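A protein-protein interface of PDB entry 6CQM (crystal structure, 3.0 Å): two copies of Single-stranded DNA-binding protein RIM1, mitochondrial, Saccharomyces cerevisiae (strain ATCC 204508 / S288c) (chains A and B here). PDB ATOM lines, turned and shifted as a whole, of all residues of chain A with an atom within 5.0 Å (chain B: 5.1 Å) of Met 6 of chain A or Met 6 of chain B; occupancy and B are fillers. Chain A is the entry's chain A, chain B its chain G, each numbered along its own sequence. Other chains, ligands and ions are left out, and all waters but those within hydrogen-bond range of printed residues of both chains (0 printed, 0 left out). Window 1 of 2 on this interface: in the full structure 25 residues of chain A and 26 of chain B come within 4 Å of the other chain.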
ATOM      1  N   SER A   4      26.053  -9.895 -26.265  1.00  0.00           N
ATOM      2  CA  SER A   4      25.195  -9.318 -25.230  1.00  0.00           C
ATOM      3  C   SER A   4      25.672  -7.884 -24.997  1.00  0.00           C
ATOM      4  O   SER A   4      26.565  -7.639 -24.184  1.00  0.00           O
ATOM      5  CB  SER A   4      25.229 -10.142 -23.951  1.00  0.00           C
ATOM      6  OG  SER A   4      26.539 -10.206 -23.417  1.00  0.00           O
ATOM      7  N   LYS A   5      25.070  -6.950 -25.724  1.00  0.00           N
ATOM      8  CA  LYS A   5      25.415  -5.540 -25.645  1.00  0.00           C
ATOM      9  C   LYS A   5      24.313  -4.775 -24.923  1.00  0.00           C
ATOM     10  O   LYS A   5      23.140  -5.160 -24.961  1.00  0.00           O
ATOM     11  CB  LYS A   5      25.637  -4.955 -27.045  1.00  0.00           C
ATOM     12  CG  LYS A   5      26.619  -3.795 -27.091  1.00  0.00           C
ATOM     13  CD  LYS A   5      26.952  -3.406 -28.524  1.00  0.00           C
ATOM     14  CE  LYS A   5      28.216  -2.562 -28.589  1.00  0.00           C
ATOM     15  NZ  LYS A   5      28.606  -2.245 -29.990  1.00  0.00           N
ATOM     16  N   MET A   6      24.701  -3.690 -24.254  1.00  0.00           N
ATOM     17  CA  MET A   6      23.766  -2.848 -23.524  1.00  0.00           C
ATOM     18  C   MET A   6      24.031  -1.385 -23.843  1.00  0.00           C
ATOM     19  O   MET A   6      25.185  -0.948 -23.886  1.00  0.00           O
ATOM     20  CB  MET A   6      23.864  -3.072 -22.007  1.00  0.00           C
ATOM     21  CG  MET A   6      22.924  -2.188 -21.197  1.00  0.00           C
ATOM     22  SD  MET A   6      23.005  -2.467 -19.421  1.00  0.00           S
ATOM     23  CE  MET A   6      22.617  -4.210 -19.334  1.00  0.00           C
ATOM     24  N   SER A   7      22.956  -0.633 -24.065  1.00  0.00           N
ATOM     25  CA  SER A   7      23.020   0.804 -24.288  1.00  0.00           C
ATOM     26  C   SER A   7      22.425   1.517 -23.081  1.00  0.00           C
ATOM     27  O   SER A   7      21.290   1.229 -22.685  1.00  0.00           O
ATOM     28  CB  SER A   7      22.273   1.196 -25.562  1.00  0.00           C
ATOM     29  OG  SER A   7      22.851   0.578 -26.700  1.00  0.00           O
ATOM     30  N   ILE A   8      23.189   2.439 -22.500  1.00  0.00           N
ATOM     31  CA  ILE A   8      22.811   3.114 -21.264  1.00  0.00           C
ATOM     32  C   ILE A   8      22.829   4.620 -21.483  1.00  0.00           C
ATOM     33  O   ILE A   8      23.765   5.160 -22.084  1.00  0.00           O
ATOM     34  CB  ILE A   8      23.745   2.730 -20.097  1.00  0.00           C
ATOM     35  CG1 ILE A   8      23.780   1.212 -19.908  1.00  0.00           C
ATOM     36  CG2 ILE A   8      23.309   3.421 -18.810  1.00  0.00           C
ATOM     37  CD1 ILE A   8      24.734   0.755 -18.824  1.00  0.00           C
ATOM     38  N   TYR A  45      24.985   1.243 -12.749  1.00  0.00           N
ATOM     39  CA  TYR A  45      25.795   0.360 -13.576  1.00  0.00           C
ATOM     40  C   TYR A  45      27.265   0.731 -13.449  1.00  0.00           C
ATOM     41  O   TYR A  45      27.620   1.913 -13.459  1.00  0.00           O
ATOM     42  CB  TYR A  45      25.365   0.427 -15.045  1.00  0.00           C
ATOM     43  CG  TYR A  45      23.947  -0.038 -15.282  1.00  0.00           C
ATOM     44  CD1 TYR A  45      23.632  -1.390 -15.282  1.00  0.00           C
ATOM     45  CD2 TYR A  45      22.924   0.875 -15.502  1.00  0.00           C
ATOM     46  CE1 TYR A  45      22.336  -1.821 -15.496  1.00  0.00           C
ATOM     47  CE2 TYR A  45      21.626   0.453 -15.718  1.00  0.00           C
ATOM     48  CZ  TYR A  45      21.338  -0.896 -15.713  1.00  0.00           C
ATOM     49  OH  TYR A  45      20.048  -1.323 -15.927  1.00  0.00           O
ATOM     50  N   VAL A  70      26.297   5.682 -23.207  1.00  0.00           N
ATOM     51  CA  VAL A  70      27.359   4.683 -23.183  1.00  0.00           C
ATOM     52  C   VAL A  70      26.840   3.396 -23.809  1.00  0.00           C
ATOM     53  O   VAL A  70      25.737   2.939 -23.484  1.00  0.00           O
ATOM     54  CB  VAL A  70      27.863   4.435 -21.751  1.00  0.00           C
ATOM     55  CG1 VAL A  70      28.854   3.281 -21.723  1.00  0.00           C
ATOM     56  CG2 VAL A  70      28.501   5.696 -21.197  1.00  0.00           C
ATOM     57  N   GLU A  71      27.634   2.819 -24.707  1.00  0.00           N
ATOM     58  CA  GLU A  71      27.359   1.516 -25.295  1.00  0.00           C
ATOM     59  C   GLU A  71      28.477   0.565 -24.896  1.00  0.00           C
ATOM     60  O   GLU A  71      29.656   0.859 -25.124  1.00  0.00           O
ATOM     61  CB  GLU A  71      27.246   1.610 -26.817  1.00  0.00           C
ATOM     62  CG  GLU A  71      26.168   0.725 -27.412  1.00  0.00           C
ATOM     63  CD  GLU A  71      25.483   1.369 -28.600  1.00  0.00           C
ATOM     64  OE1 GLU A  71      26.156   2.112 -29.345  1.00  0.00           O
ATOM     65  OE2 GLU A  71      24.270   1.133 -28.786  1.00  0.00           O
ATOM     66  N   ALA A  72      28.111  -0.566 -24.296  1.00  0.00           N
ATOM     67  CA  ALA A  72      29.092  -1.468 -23.715  1.00  0.00           C
ATOM     68  C   ALA A  72      28.711  -2.914 -23.988  1.00  0.00           C
ATOM     69  O   ALA A  72      27.530  -3.256 -24.085  1.00  0.00           O
ATOM     70  CB  ALA A  72      29.227  -1.245 -22.203  1.00  0.00           C
ATOM     71  N   ALA A  74      28.212  -6.436 -22.584  1.00  0.00           N
ATOM     72  CA  ALA A  74      27.886  -6.976 -21.273  1.00  0.00           C
ATOM     73  C   ALA A  74      28.407  -8.399 -21.130  1.00  0.00           C
ATOM     74  O   ALA A  74      28.313  -9.208 -22.057  1.00  0.00           O
ATOM     75  CB  ALA A  74      26.374  -6.949 -21.041  1.00  0.00           C
ATOM     76  N   LEU A  90      28.202  -8.634 -13.095  1.00  0.00           N
ATOM     77  CA  LEU A  90      27.916  -8.074 -14.409  1.00  0.00           C
ATOM     78  C   LEU A  90      29.042  -7.130 -14.813  1.00  0.00           C
ATOM     79  O   LEU A  90      29.330  -6.159 -14.105  1.00  0.00           O
ATOM     80  CB  LEU A  90      26.574  -7.342 -14.404  1.00  0.00           C
ATOM     81  CG  LEU A  90      26.185  -6.619 -15.696  1.00  0.00           C
ATOM     82  CD1 LEU A  90      26.070  -7.604 -16.850  1.00  0.00           C
ATOM     83  CD2 LEU A  90      24.885  -5.850 -15.512  1.00  0.00           C
ATOM     84  N   LEU A  92      30.585  -4.531 -17.768  1.00  0.00           N
ATOM     85  CA  LEU A  92      30.171  -3.650 -18.859  1.00  0.00           C
ATOM     86  C   LEU A  92      31.416  -2.946 -19.394  1.00  0.00           C
ATOM     87  O   LEU A  92      31.840  -1.923 -18.850  1.00  0.00           O
ATOM     88  CB  LEU A  92      29.122  -2.646 -18.389  1.00  0.00           C
ATOM     89  CG  LEU A  92      27.814  -3.233 -17.851  1.00  0.00           C
ATOM     90  CD1 LEU A  92      26.894  -2.133 -17.347  1.00  0.00           C
ATOM     91  CD2 LEU A  92      27.118  -4.066 -18.913  1.00  0.00           C
ATOM     92  N   SER B   4      18.044   1.749 -20.053  1.00  0.00           N
ATOM     93  CA  SER B   4      19.103   0.739 -20.061  1.00  0.00           C
ATOM     94  C   SER B   4      18.542  -0.483 -20.792  1.00  0.00           C
ATOM     95  O   SER B   4      17.901  -1.344 -20.187  1.00  0.00           O
ATOM     96  CB  SER B   4      19.565   0.396 -18.653  1.00  0.00           C
ATOM     97  OG  SER B   4      18.487  -0.056 -17.854  1.00  0.00           O
ATOM     98  N   LYS B   5      18.784  -0.535 -22.099  1.00  0.00           N
ATOM     99  CA  LYS B   5      18.302  -1.615 -22.948  1.00  0.00           C
ATOM    100  C   LYS B   5      19.400  -2.646 -23.160  1.00  0.00           C
ATOM    101  O   LYS B   5      20.576  -2.297 -23.296  1.00  0.00           O
ATOM    102  CB  LYS B   5      17.831  -1.079 -24.301  1.00  0.00           C
ATOM    103  CG  LYS B   5      16.824   0.051 -24.209  1.00  0.00           C
ATOM    104  CD  LYS B   5      15.522  -0.411 -23.583  1.00  0.00           C
ATOM    105  CE  LYS B   5      14.403   0.585 -23.842  1.00  0.00           C
ATOM    106  NZ  LYS B   5      13.089   0.072 -23.369  1.00  0.00           N
ATOM    107  N   MET B   6      19.007  -3.915 -23.205  1.00  0.00           N
ATOM    108  CA  MET B   6      19.932  -5.023 -23.394  1.00  0.00           C
ATOM    109  C   MET B   6      19.507  -5.836 -24.608  1.00  0.00           C
ATOM    110  O   MET B   6      18.338  -6.219 -24.725  1.00  0.00           O
ATOM    111  CB  MET B   6      19.979  -5.912 -22.150  1.00  0.00           C
ATOM    112  CG  MET B   6      20.867  -7.132 -22.292  1.00  0.00           C
ATOM    113  SD  MET B   6      22.528  -6.904 -21.631  1.00  0.00           S
ATOM    114  CE  MET B   6      23.061  -8.601 -21.506  1.00  0.00           C
ATOM    115  N   SER B   7      20.454  -6.092 -25.505  1.00  0.00           N
ATOM    116  CA  SER B   7      20.236  -6.915 -26.688  1.00  0.00           C
ATOM    117  C   SER B   7      21.068  -8.183 -26.555  1.00  0.00           C
ATOM    118  O   SER B   7      22.297  -8.112 -26.439  1.00  0.00           O
ATOM    119  CB  SER B   7      20.608  -6.154 -27.960  1.00  0.00           C
ATOM    120  OG  SER B   7      19.807  -4.997 -28.112  1.00  0.00           O
ATOM    121  N   ILE B   8      20.403  -9.336 -26.571  1.00  0.00           N
ATOM    122  CA  ILE B   8      21.052 -10.619 -26.326  1.00  0.00           C
ATOM    123  C   ILE B   8      20.754 -11.557 -27.486  1.00  0.00           C
ATOM    124  O   ILE B   8      19.597 -11.697 -27.897  1.00  0.00           O
ATOM    125  CB  ILE B   8      20.586 -11.254 -25.001  1.00  0.00           C
ATOM    126  CG1 ILE B   8      20.770 -10.279 -23.841  1.00  0.00           C
ATOM    127  CG2 ILE B   8      21.347 -12.542 -24.732  1.00  0.00           C
ATOM    128  CD1 ILE B   8      20.258 -10.805 -22.517  1.00  0.00           C
ATOM    129  N   TYR B  45      22.209 -15.245 -18.582  1.00  0.00           N
ATOM    130  CA  TYR B  45      21.321 -14.149 -18.227  1.00  0.00           C
ATOM    131  C   TYR B  45      19.945 -14.694 -17.877  1.00  0.00           C
ATOM    132  O   TYR B  45      19.410 -15.556 -18.581  1.00  0.00           O
ATOM    133  CB  TYR B  45      21.200 -13.135 -19.369  1.00  0.00           C
ATOM    134  CG  TYR B  45      22.509 -12.486 -19.742  1.00  0.00           C
ATOM    135  CD1 TYR B  45      23.095 -11.537 -18.916  1.00  0.00           C
ATOM    136  CD2 TYR B  45      23.161 -12.822 -20.921  1.00  0.00           C
ATOM    137  CE1 TYR B  45      24.295 -10.944 -19.250  1.00  0.00           C
ATOM    138  CE2 TYR B  45      24.360 -12.233 -21.265  1.00  0.00           C
ATOM    139  CZ  TYR B  45      24.922 -11.294 -20.427  1.00  0.00           C
ATOM    140  OH  TYR B  45      26.118 -10.700 -20.764  1.00  0.00           O
ATOM    141  N   VAL B  70      16.852 -11.363 -28.209  1.00  0.00           N
ATOM    142  CA  VAL B  70      15.963 -10.787 -27.207  1.00  0.00           C
ATOM    143  C   VAL B  70      16.381  -9.346 -26.943  1.00  0.00           C
ATOM    144  O   VAL B  70      17.570  -9.062 -26.761  1.00  0.00           O
ATOM    145  CB  VAL B  70      15.983 -11.605 -25.903  1.00  0.00           C
ATOM    146  CG1 VAL B  70      15.141 -10.931 -24.831  1.00  0.00           C
ATOM    147  CG2 VAL B  70      15.498 -13.023 -26.160  1.00  0.00           C
ATOM    148  N   GLU B  71      15.404  -8.444 -26.932  1.00  0.00           N
ATOM    149  CA  GLU B  71      15.582  -7.083 -26.445  1.00  0.00           C
ATOM    150  C   GLU B  71      14.898  -6.963 -25.092  1.00  0.00           C
ATOM    151  O   GLU B  71      13.701  -7.251 -24.971  1.00  0.00           O
ATOM    152  CB  GLU B  71      15.006  -6.055 -27.422  1.00  0.00           C
ATOM    153  CG  GLU B  71      15.789  -5.907 -28.712  1.00  0.00           C
ATOM    154  CD  GLU B  71      15.316  -4.732 -29.544  1.00  0.00           C
ATOM    155  OE1 GLU B  71      15.746  -3.594 -29.263  1.00  0.00           O
ATOM    156  OE2 GLU B  71      14.511  -4.945 -30.476  1.00  0.00           O
ATOM    157  N   ALA B  72      15.652  -6.543 -24.078  1.00  0.00           N
ATOM    158  CA  ALA B  72      15.145  -6.519 -22.715  1.00  0.00           C
ATOM    159  C   ALA B  72      15.539  -5.223 -22.025  1.00  0.00           C
ATOM    160  O   ALA B  72      16.646  -4.715 -22.222  1.00  0.00           O
ATOM    161  CB  ALA B  72      15.666  -7.714 -21.906  1.00  0.00           C
ATOM    162  N   ASP B  73      14.624  -4.694 -21.214  1.00  0.00           N
ATOM    163  CA  ASP B  73      14.936  -3.563 -20.353  1.00  0.00           C
ATOM    164  C   ASP B  73      15.726  -4.052 -19.148  1.00  0.00           C
ATOM    165  O   ASP B  73      15.305  -4.983 -18.456  1.00  0.00           O
ATOM    166  CB  ASP B  73      13.658  -2.859 -19.897  1.00  0.00           C
ATOM    167  CG  ASP B  73      12.934  -2.169 -21.034  1.00  0.00           C
ATOM    168  OD1 ASP B  73      13.397  -2.276 -22.189  1.00  0.00           O
ATOM    169  OD2 ASP B  73      11.906  -1.509 -20.771  1.00  0.00           O
ATOM    170  N   ALA B  74      16.873  -3.427 -18.901  1.00  0.00           N
ATOM    171  CA  ALA B  74      17.764  -3.837 -17.827  1.00  0.00           C
ATOM    172  C   ALA B  74      17.577  -2.942 -16.610  1.00  0.00           C
ATOM    173  O   ALA B  74      17.466  -1.719 -16.735  1.00  0.00           O
ATOM    174  CB  ALA B  74      19.222  -3.794 -18.283  1.00  0.00           C
ATOM    175  N   LEU B  92      16.205  -8.322 -15.950  1.00  0.00           N
ATOM    176  CA  LEU B  92      16.139  -8.287 -17.411  1.00  0.00           C
ATOM    177  C   LEU B  92      14.714  -8.642 -17.827  1.00  0.00           C
ATOM    178  O   LEU B  92      14.358  -9.822 -17.908  1.00  0.00           O
ATOM    179  CB  LEU B  92      17.154  -9.241 -18.036  1.00  0.00           C
ATOM    180  CG  LEU B  92      18.633  -8.912 -17.821  1.00  0.00           C
ATOM    181  CD1 LEU B  92      19.515  -9.981 -18.447  1.00  0.00           C
ATOM    182  CD2 LEU B  92      18.965  -7.542 -18.393  1.00  0.00           C
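N of Ser 7 of chain A sits at hydrogen-bond distance from O of Lys 5 of chain B (3.0 Å). The side-chain hydroxyl (OG) of Ser 4 of chain B is in hydrogen-bond range of the side-chain hydroxyl (OH) of Tyr 45 of chain A. The side-chain hydroxyl of Tyr 45 of chain A is in hydrogen-bond range of the backbone carbonyl oxygen of Ala 74 of chain B, 2.7 Å away. O of Lys 5 of chain A sits at hydrogen-bond distance from N of Ser 7 of chain B, at 2.9 Å. The side-chain hydroxyl of Ser 4 of chain A lies within hydrogen-bond range of the side-chain hydroxyl of Tyr 45 of chain B. The side-chain hydroxyl (OH) of Tyr 45 of chain B sits at hydrogen-bond distance from the backbone carbonyl oxygen (O) of Ala 74 of chain A (3.0 Å).
O of Ser 4 of chain B lies within hydrogen-bond range of N of Ala 74 of chain B, at 2.7 Å. The side-chain carboxylate (OE2) of Glu 71 of chain A is in hydrogen-bond range of the side-chain hydroxyl (OG) of Ser 7 of chain A (2.6 Å). The backbone carbonyl oxygen (O) of Ala 72 of chain A is in hydrogen-bond range of the backbone NH (N) of Met 6 of chain A, at 2.9 Å. O of Ala 74 of chain A lies within hydrogen-bond range of OG of Ser 4 of chain A (2.4 Å). The backbone carbonyl oxygen (O) of Ala 72 of chain B lies within hydrogen-bond range of the backbone NH (N) of Met 6 of chain B (2.7 Å). The side-chain amino group of Lys 5 of chain B is in salt-bridge range of the side-chain carboxylate of Asp 73 of chain B, at 2.6 Å.
Among the printed residues, merely in contact across the chains: Ser 4 of chain A with Met 6 of chain B, Ser 4 of chain A with Ser 7 of chain B, Lys 5 of chain A with Met 6 of chain B, Met 6 of chain A with Lys 5 of chain B, Met 6 of chain A with Met 6 of chain B, Met 6 of chain A with Ala 74 of chain B, Ser 7 of chain A with Ser 4 of chain B and Ala 74 of chain A with Met 6 of chain B.
Met 6 of chain A touches just these residues of chain B: Lys 5, Met 6 and Ala 74. Of chain A, only Ser 4 (3.6 Å), Lys 5 (3.6 Å), Met 6 (3.5 Å) and Ala 74 (3.7 Å) come within 4 Å of Met 6 of chain B. Of the printed residues of chain A, Ser 7 of chain B touches Ser 4 and Lys 5. Of the printed residues of chain B, Tyr 45 of chain A touches Ser 4 and Ala 74. Of the printed residues of chain A, Ala 74 of chain B touches Met 6 (3.6 Å) and Tyr 45 (2.7 Å). The nearest printed residue of chain A that does not touch Ser 4 of chain B is Ile 8 of chain A (4.5 Å).
Of the 12 printed residues of chain B, 6 touch a printed residue of chain A. Hydrophobic or aromatic side chains of chain B that line the printed part of chain A: Met 6, Tyr 45 and Ala 74. Hydrophobic or aromatic side chains of chain A that line the printed part of chain B: Met 6, Tyr 45 and Ala 74.
Ser 4 of chain A touches Met 6 of chain B, but with the chains exchanged Met 6 of chain A does not touch Ser 4 of chain B (4.5 Å). Ser 4 of chain A touches Ser 7 of chain B, and with the chains exchanged Ser 7 of chain A touches Ser 4 of chain B. Ser 4 of chain A touches Tyr 45 of chain B, and with the chains exchanged Tyr 45 of chain A touches Ser 4 of chain B. Met 6 of chain B touches its own counterpart, Met 6 of chain A.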
